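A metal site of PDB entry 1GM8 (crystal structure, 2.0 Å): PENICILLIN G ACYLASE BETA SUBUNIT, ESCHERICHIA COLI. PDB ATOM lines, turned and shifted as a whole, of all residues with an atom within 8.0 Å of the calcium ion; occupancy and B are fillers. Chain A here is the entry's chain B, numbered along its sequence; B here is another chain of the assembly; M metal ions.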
ATOM      1  N   GLY A  72      26.218   2.930  27.961  1.00  0.00           N
ATOM      2  CA  GLY A  72      25.210   1.917  28.277  1.00  0.00           C
ATOM      3  C   GLY A  72      24.878   1.155  26.975  1.00  0.00           C
ATOM      4  O   GLY A  72      25.206   1.606  25.903  1.00  0.00           O
ATOM      5  N   ASP A  73      24.230   0.003  27.065  1.00  0.00           N
ATOM      6  CA  ASP A  73      23.863  -0.740  25.872  1.00  0.00           C
ATOM      7  C   ASP A  73      22.460  -0.289  25.425  1.00  0.00           C
ATOM      8  O   ASP A  73      21.499  -0.870  25.939  1.00  0.00           O
ATOM      9  CB  ASP A  73      23.796  -2.197  26.298  1.00  0.00           C
ATOM     10  CG  ASP A  73      23.613  -3.049  25.102  1.00  0.00           C
ATOM     11  OD1 ASP A  73      23.212  -2.446  24.124  1.00  0.00           O
ATOM     12  OD2 ASP A  73      23.784  -4.243  24.987  1.00  0.00           O
ATOM     13  N   ASP A  74      22.423   0.686  24.504  1.00  0.00           N
ATOM     14  CA  ASP A  74      21.136   1.190  24.033  1.00  0.00           C
ATOM     15  C   ASP A  74      20.909   0.769  22.565  1.00  0.00           C
ATOM     16  O   ASP A  74      20.111   1.358  21.859  1.00  0.00           O
ATOM     17  CB  ASP A  74      21.149   2.695  24.132  1.00  0.00           C
ATOM     18  CG  ASP A  74      22.262   3.468  23.479  1.00  0.00           C
ATOM     19  OD1 ASP A  74      23.212   2.856  23.028  1.00  0.00           O
ATOM     20  OD2 ASP A  74      22.187   4.755  23.384  1.00  0.00           O
ATOM     21  N   VAL A  75      21.744  -0.174  22.088  1.00  0.00           N
ATOM     22  CA  VAL A  75      21.684  -0.599  20.705  1.00  0.00           C
ATOM     23  C   VAL A  75      21.502  -2.078  20.555  1.00  0.00           C
ATOM     24  O   VAL A  75      22.500  -2.629  21.008  1.00  0.00           O
ATOM     25  CB  VAL A  75      22.901  -0.169  19.831  1.00  0.00           C
ATOM     26  CG1 VAL A  75      22.697  -0.673  18.393  1.00  0.00           C
ATOM     27  CG2 VAL A  75      22.928   1.345  19.809  1.00  0.00           C
ATOM     28  N   ASP A  76      20.630  -2.745  19.869  1.00  0.00           N
ATOM     29  CA  ASP A  76      20.624  -4.166  19.642  1.00  0.00           C
ATOM     30  C   ASP A  76      20.387  -4.373  18.118  1.00  0.00           C
ATOM     31  O   ASP A  76      19.849  -3.494  17.399  1.00  0.00           O
ATOM     32  CB  ASP A  76      19.504  -4.981  20.336  1.00  0.00           C
ATOM     33  CG  ASP A  76      19.395  -4.863  21.828  1.00  0.00           C
ATOM     34  OD1 ASP A  76      20.390  -4.655  22.530  1.00  0.00           O
ATOM     35  OD2 ASP A  76      18.394  -4.946  22.575  1.00  0.00           O
ATOM     36  N   ILE A  77      20.879  -5.527  17.678  1.00  0.00           N
ATOM     37  CA  ILE A  77      20.712  -5.963  16.315  1.00  0.00           C
ATOM     38  C   ILE A  77      19.647  -7.047  16.173  1.00  0.00           C
ATOM     39  O   ILE A  77      19.643  -8.148  16.798  1.00  0.00           O
ATOM     40  CB  ILE A  77      22.015  -6.550  15.778  1.00  0.00           C
ATOM     41  CG1 ILE A  77      23.188  -5.553  15.914  1.00  0.00           C
ATOM     42  CG2 ILE A  77      21.858  -7.040  14.338  1.00  0.00           C
ATOM     43  CD1 ILE A  77      23.089  -4.337  15.021  1.00  0.00           C
ATOM     44  N   SER A 140      18.877  -1.559  15.784  1.00  0.00           N
ATOM     45  CA  SER A 140      17.839  -0.862  16.519  1.00  0.00           C
ATOM     46  C   SER A 140      18.388   0.028  17.650  1.00  0.00           C
ATOM     47  O   SER A 140      19.055  -0.453  18.614  1.00  0.00           O
ATOM     48  CB  SER A 140      16.947  -1.991  17.016  1.00  0.00           C
ATOM     49  OG  SER A 140      15.781  -1.589  17.671  1.00  0.00           O
ATOM     50  N   PRO A 197      16.086   0.022  26.266  1.00  0.00           N
ATOM     51  CA  PRO A 197      14.965  -0.776  25.898  1.00  0.00           C
ATOM     52  C   PRO A 197      14.496  -1.686  27.006  1.00  0.00           C
ATOM     53  O   PRO A 197      15.332  -2.146  27.757  1.00  0.00           O
ATOM     54  CB  PRO A 197      15.424  -1.650  24.716  1.00  0.00           C
ATOM     55  CG  PRO A 197      16.950  -1.722  24.921  1.00  0.00           C
ATOM     56  CD  PRO A 197      17.381  -0.406  25.601  1.00  0.00           C
ATOM     57  N   ARG A 199      13.739  -5.139  27.541  1.00  0.00           N
ATOM     58  CA  ARG A 199      13.818  -6.317  26.655  1.00  0.00           C
ATOM     59  C   ARG A 199      12.993  -7.478  27.196  1.00  0.00           C
ATOM     60  O   ARG A 199      12.706  -7.568  28.382  1.00  0.00           O
ATOM     61  CB  ARG A 199      15.284  -6.733  26.613  1.00  0.00           C
ATOM     62  CG  ARG A 199      16.182  -5.676  25.945  1.00  0.00           C
ATOM     63  CD  ARG A 199      17.639  -6.049  26.103  1.00  0.00           C
ATOM     64  NE  ARG A 199      18.582  -5.190  25.294  1.00  0.00           N
ATOM     65  CZ  ARG A 199      19.277  -4.246  25.898  1.00  0.00           C
ATOM     66  NH1 ARG A 199      19.186  -3.966  27.194  1.00  0.00           N
ATOM     67  NH2 ARG A 199      20.144  -3.500  25.203  1.00  0.00           N
ATOM     68  N   HIS A 203      16.356 -12.312  26.783  1.00  0.00           N
ATOM     69  CA  HIS A 203      17.173 -11.562  25.821  1.00  0.00           C
ATOM     70  C   HIS A 203      18.560 -11.139  26.326  1.00  0.00           C
ATOM     71  O   HIS A 203      18.671 -10.304  27.222  1.00  0.00           O
ATOM     72  CB  HIS A 203      16.358 -10.344  25.352  1.00  0.00           C
ATOM     73  CG  HIS A 203      16.907  -9.430  24.343  1.00  0.00           C
ATOM     74  ND1 HIS A 203      18.209  -9.368  23.875  1.00  0.00           N
ATOM     75  CD2 HIS A 203      16.263  -8.421  23.706  1.00  0.00           C
ATOM     76  CE1 HIS A 203      18.285  -8.362  23.013  1.00  0.00           C
ATOM     77  NE2 HIS A 203      17.088  -7.733  22.893  1.00  0.00           N
ATOM     78  N   ASP A 204      19.561 -11.813  25.804  1.00  0.00           N
ATOM     79  CA  ASP A 204      20.979 -11.527  26.136  1.00  0.00           C
ATOM     80  C   ASP A 204      21.365 -10.311  25.260  1.00  0.00           C
ATOM     81  O   ASP A 204      21.425 -10.362  24.017  1.00  0.00           O
ATOM     82  CB  ASP A 204      21.794 -12.731  25.668  1.00  0.00           C
ATOM     83  CG  ASP A 204      23.246 -12.622  26.180  1.00  0.00           C
ATOM     84  OD1 ASP A 204      23.741 -11.473  26.221  1.00  0.00           O
ATOM     85  OD2 ASP A 204      23.813 -13.724  26.418  1.00  0.00           O
ATOM     86  N   PRO A 205      21.623  -9.194  25.837  1.00  0.00           N
ATOM     87  CA  PRO A 205      21.873  -7.948  25.118  1.00  0.00           C
ATOM     88  C   PRO A 205      23.213  -7.934  24.454  1.00  0.00           C
ATOM     89  O   PRO A 205      23.443  -6.996  23.689  1.00  0.00           O
ATOM     90  CB  PRO A 205      21.752  -6.792  26.152  1.00  0.00           C
ATOM     91  CG  PRO A 205      22.056  -7.535  27.441  1.00  0.00           C
ATOM     92  CD  PRO A 205      21.627  -9.003  27.303  1.00  0.00           C
ATOM     93  N   ARG A 206      24.112  -8.908  24.581  1.00  0.00           N
ATOM     94  CA  ARG A 206      25.355  -8.802  23.852  1.00  0.00           C
ATOM     95  C   ARG A 206      25.201  -9.414  22.481  1.00  0.00           C
ATOM     96  O   ARG A 206      26.174  -9.342  21.674  1.00  0.00           O
ATOM     97  CB  ARG A 206      26.434  -9.560  24.695  1.00  0.00           C
ATOM     98  CG  ARG A 206      26.539  -8.959  26.135  1.00  0.00           C
ATOM     99  CD  ARG A 206      27.286  -9.991  27.010  1.00  0.00           C
ATOM    100  NE  ARG A 206      26.512 -11.256  27.123  1.00  0.00           N
ATOM    101  CZ  ARG A 206      26.965 -12.287  27.834  1.00  0.00           C
ATOM    102  NH1 ARG A 206      28.186 -12.201  28.399  1.00  0.00           N
ATOM    103  NH2 ARG A 206      26.268 -13.388  27.875  1.00  0.00           N
ATOM    104  N   LEU A 207      24.096 -10.106  22.178  1.00  0.00           N
ATOM    105  CA  LEU A 207      24.036 -10.790  20.868  1.00  0.00           C
ATOM    106  C   LEU A 207      22.706 -10.538  20.145  1.00  0.00           C
ATOM    107  O   LEU A 207      21.694 -10.224  20.775  1.00  0.00           O
ATOM    108  CB  LEU A 207      24.177 -12.263  21.244  1.00  0.00           C
ATOM    109  CG  LEU A 207      25.446 -12.701  21.955  1.00  0.00           C
ATOM    110  CD1 LEU A 207      25.195 -13.879  22.890  1.00  0.00           C
ATOM    111  CD2 LEU A 207      26.461 -12.983  20.839  1.00  0.00           C
ATOM    112  N   PRO A 208      22.621 -10.776  18.860  1.00  0.00           N
ATOM    113  CA  PRO A 208      21.474 -10.400  18.003  1.00  0.00           C
ATOM    114  C   PRO A 208      20.236 -11.122  18.406  1.00  0.00           C
ATOM    115  O   PRO A 208      20.370 -12.172  19.042  1.00  0.00           O
ATOM    116  CB  PRO A 208      21.859 -10.765  16.547  1.00  0.00           C
ATOM    117  CG  PRO A 208      23.362 -10.865  16.593  1.00  0.00           C
ATOM    118  CD  PRO A 208      23.744 -11.226  18.015  1.00  0.00           C
ATOM    119  N   VAL A 209      19.066 -10.503  18.149  1.00  0.00           N
ATOM    120  CA  VAL A 209      17.822 -11.195  18.439  1.00  0.00           C
ATOM    121  C   VAL A 209      17.040 -11.476  17.142  1.00  0.00           C
ATOM    122  O   VAL A 209      17.102 -10.713  16.178  1.00  0.00           O
ATOM    123  CB  VAL A 209      16.920 -10.322  19.346  1.00  0.00           C
ATOM    124  CG1 VAL A 209      17.150 -10.741  20.790  1.00  0.00           C
ATOM    125  CG2 VAL A 209      17.146  -8.816  19.207  1.00  0.00           C
ATOM    126  N   TRP A 217      11.539  -5.450  21.399  1.00  0.00           N
ATOM    127  CA  TRP A 217      11.492  -4.769  22.694  1.00  0.00           C
ATOM    128  C   TRP A 217      10.044  -4.550  23.123  1.00  0.00           C
ATOM    129  O   TRP A 217       9.105  -4.303  22.368  1.00  0.00           O
ATOM    130  CB  TRP A 217      12.190  -3.440  22.455  1.00  0.00           C
ATOM    131  CG  TRP A 217      13.683  -3.543  22.238  1.00  0.00           C
ATOM    132  CD1 TRP A 217      14.554  -4.568  22.533  1.00  0.00           C
ATOM    133  CD2 TRP A 217      14.477  -2.463  21.702  1.00  0.00           C
ATOM    134  NE1 TRP A 217      15.854  -4.188  22.168  1.00  0.00           N
ATOM    135  CE2 TRP A 217      15.801  -2.918  21.644  1.00  0.00           C
ATOM    136  CE3 TRP A 217      14.159  -1.169  21.271  1.00  0.00           C
ATOM    137  CZ2 TRP A 217      16.833  -2.069  21.266  1.00  0.00           C
ATOM    138  CZ3 TRP A 217      15.189  -0.369  20.800  1.00  0.00           C
ATOM    139  CH2 TRP A 217      16.552  -0.817  20.818  1.00  0.00           C
ATOM    140  N   ALA A 250      27.392  -2.689  30.718  1.00  0.00           N
ATOM    141  CA  ALA A 250      28.073  -1.904  29.735  1.00  0.00           C
ATOM    142  C   ALA A 250      27.537  -2.145  28.306  1.00  0.00           C
ATOM    143  O   ALA A 250      26.904  -3.165  28.001  1.00  0.00           O
ATOM    144  CB  ALA A 250      29.557  -2.443  29.713  1.00  0.00           C
ATOM    145  N   SER A 251      27.944  -1.238  27.444  1.00  0.00           N
ATOM    146  CA  SER A 251      27.785  -1.374  25.967  1.00  0.00           C
ATOM    147  C   SER A 251      28.186  -2.770  25.504  1.00  0.00           C
ATOM    148  O   SER A 251      29.039  -3.408  26.166  1.00  0.00           O
ATOM    149  CB  SER A 251      28.918  -0.443  25.421  1.00  0.00           C
ATOM    150  OG  SER A 251      29.105  -0.673  24.037  1.00  0.00           O
ATOM    151  N   ASP A 252      27.585  -3.376  24.472  1.00  0.00           N
ATOM    152  CA  ASP A 252      27.966  -4.728  24.089  1.00  0.00           C
ATOM    153  C   ASP A 252      29.241  -4.792  23.238  1.00  0.00           C
ATOM    154  O   ASP A 252      29.634  -5.877  22.904  1.00  0.00           O
ATOM    155  CB  ASP A 252      26.759  -5.348  23.323  1.00  0.00           C
ATOM    156  CG  ASP A 252      26.565  -4.616  22.018  1.00  0.00           C
ATOM    157  OD1 ASP A 252      27.481  -4.322  21.229  1.00  0.00           O
ATOM    158  OD2 ASP A 252      25.453  -4.313  21.581  1.00  0.00           O
ATOM    159  N   LEU A 253      29.966  -3.731  22.973  1.00  0.00           N
ATOM    160  CA  LEU A 253      31.208  -3.748  22.200  1.00  0.00           C
ATOM    161  C   LEU A 253      32.151  -4.813  22.811  1.00  0.00           C
ATOM    162  O   LEU A 253      32.544  -4.712  23.972  1.00  0.00           O
ATOM    163  CB  LEU A 253      31.905  -2.400  22.209  1.00  0.00           C
ATOM    164  CG  LEU A 253      31.209  -1.214  21.558  1.00  0.00           C
ATOM    165  CD1 LEU A 253      32.054   0.014  21.829  1.00  0.00           C
ATOM    166  CD2 LEU A 253      31.045  -1.552  20.063  1.00  0.00           C
ATOM    167  N   SER B 149      26.918   2.526  19.428  1.00  0.00           N
ATOM    168  CA  SER B 149      27.969   1.489  19.312  1.00  0.00           C
ATOM    169  C   SER B 149      27.384   0.115  19.660  1.00  0.00           C
ATOM    170  O   SER B 149      26.841  -0.077  20.734  1.00  0.00           O
ATOM    171  CB  SER B 149      28.990   1.754  20.462  1.00  0.00           C
ATOM    172  OG  SER B 149      29.676   2.938  20.268  1.00  0.00           O
ATOM    173  N   THR B 150      27.566  -0.825  18.762  1.00  0.00           N
ATOM    174  CA  THR B 150      27.190  -2.195  18.902  1.00  0.00           C
ATOM    175  C   THR B 150      28.230  -3.063  18.143  1.00  0.00           C
ATOM    176  O   THR B 150      28.743  -2.605  17.147  1.00  0.00           O
ATOM    177  CB  THR B 150      25.781  -2.535  18.493  1.00  0.00           C
ATOM    178  OG1 THR B 150      25.493  -3.888  18.920  1.00  0.00           O
ATOM    179  CG2 THR B 150      25.543  -2.453  16.946  1.00  0.00           C
ATOM    180  N   SER B 151      28.551  -4.258  18.672  1.00  0.00           N
ATOM    181  CA  SER B 151      29.454  -5.142  17.889  1.00  0.00           C
ATOM    182  C   SER B 151      28.762  -6.486  17.940  1.00  0.00           C
ATOM    183  O   SER B 151      29.411  -7.553  17.840  1.00  0.00           O
ATOM    184  CB  SER B 151      30.855  -5.211  18.512  1.00  0.00           C
ATOM    185  OG  SER B 151      30.811  -5.855  19.812  1.00  0.00           O
ATOM    186  N   GLU B 152      27.406  -6.487  18.086  1.00  0.00           N
ATOM    187  CA  GLU B 152      26.749  -7.790  18.280  1.00  0.00           C
ATOM    188  C   GLU B 152      26.999  -8.846  17.192  1.00  0.00           C
ATOM    189  O   GLU B 152      26.931 -10.039  17.524  1.00  0.00           O
ATOM    190  CB  GLU B 152      25.191  -7.652  18.440  1.00  0.00           C
ATOM    191  CG  GLU B 152      24.744  -7.035  19.801  1.00  0.00           C
ATOM    192  CD  GLU B 152      23.265  -6.921  19.808  1.00  0.00           C
ATOM    193  OE1 GLU B 152      22.590  -7.449  18.920  1.00  0.00           O
ATOM    194  OE2 GLU B 152      22.600  -6.307  20.658  1.00  0.00           O
ATOM    195  N   ASN B 155      30.243 -10.167  18.012  1.00  0.00           N
ATOM    196  CA  ASN B 155      30.154 -10.995  19.200  1.00  0.00           C
ATOM    197  C   ASN B 155      29.664 -12.414  18.906  1.00  0.00           C
ATOM    198  O   ASN B 155      30.070 -13.426  19.568  1.00  0.00           O
ATOM    199  CB  ASN B 155      29.204 -10.382  20.288  1.00  0.00           C
ATOM    200  CG  ASN B 155      29.705  -8.996  20.703  1.00  0.00           C
ATOM    201  OD1 ASN B 155      30.808  -8.572  20.352  1.00  0.00           O
ATOM    202  ND2 ASN B 155      28.866  -8.269  21.411  1.00  0.00           N
HETATM  203 CA    CA M   1      22.995  -4.684  22.505  1.00  0.00          CA
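The calcium ion is bound by the side-chain carboxylate (OE2) of Glu 152 of chain B (2.5 Å), the backbone carbonyl oxygen (O) of Val 75 (2.6 Å), the side-chain carboxylate (OD1) of Asp 76 (2.6 Å), the backbone carbonyl oxygen (O) of Pro 205 (2.6 Å), the side-chain carboxylate (OD2) of Asp 73 (2.6 Å), the side-chain carboxylate (OD2) of Asp 252 (2.7 Å) and the side-chain carboxylate (OD1) of Asp 73 (2.8 Å).
The calcium ion has seven donor atoms within binding distance.
Six residues have an atom within 4 Å of the calcium ion: Asp 73, Val 75, Asp 76, Pro 205, Asp 252 and Glu 152 of chain B.
Along chain A the residues within 4 Å of the calcium ion span positions 73 to 252.
The nearest printed residue that does not touch the calcium ion is Arg 199 (4.1 Å).
The backbone carbonyl oxygen (O) of Asp 73 is in hydrogen-bond range of the guanidinium group (NH2) of Arg 199.
The backbone NH of Glu 152 of chain B lies within hydrogen-bond range of the side-chain hydroxyl of Thr 150 of chain B.
OD2 of Asp 76 is in hydrogen-bond range of NE1 of Trp 217 (2.7 Å).
The backbone carbonyl oxygen of Asp 76 is in hydrogen-bond range of the backbone NH of Ser 140, at 2.7 Å.
OD2 of Asp 76 sits at hydrogen-bond distance from NE2 of His 203, 3.1 Å away.
The side-chain carboxylate (OE1) of Glu 152 of chain B lies within hydrogen-bond range of the backbone NH (N) of Ile 77 (2.9 Å).
OD1 of Asp 252 lies within hydrogen-bond range of OG1 of Thr 150 of chain B.
The guanidinium group (NE) of Arg 199 lies within salt-bridge range of the side-chain carboxylate (OD2) of Asp 76 (2.7 Å).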
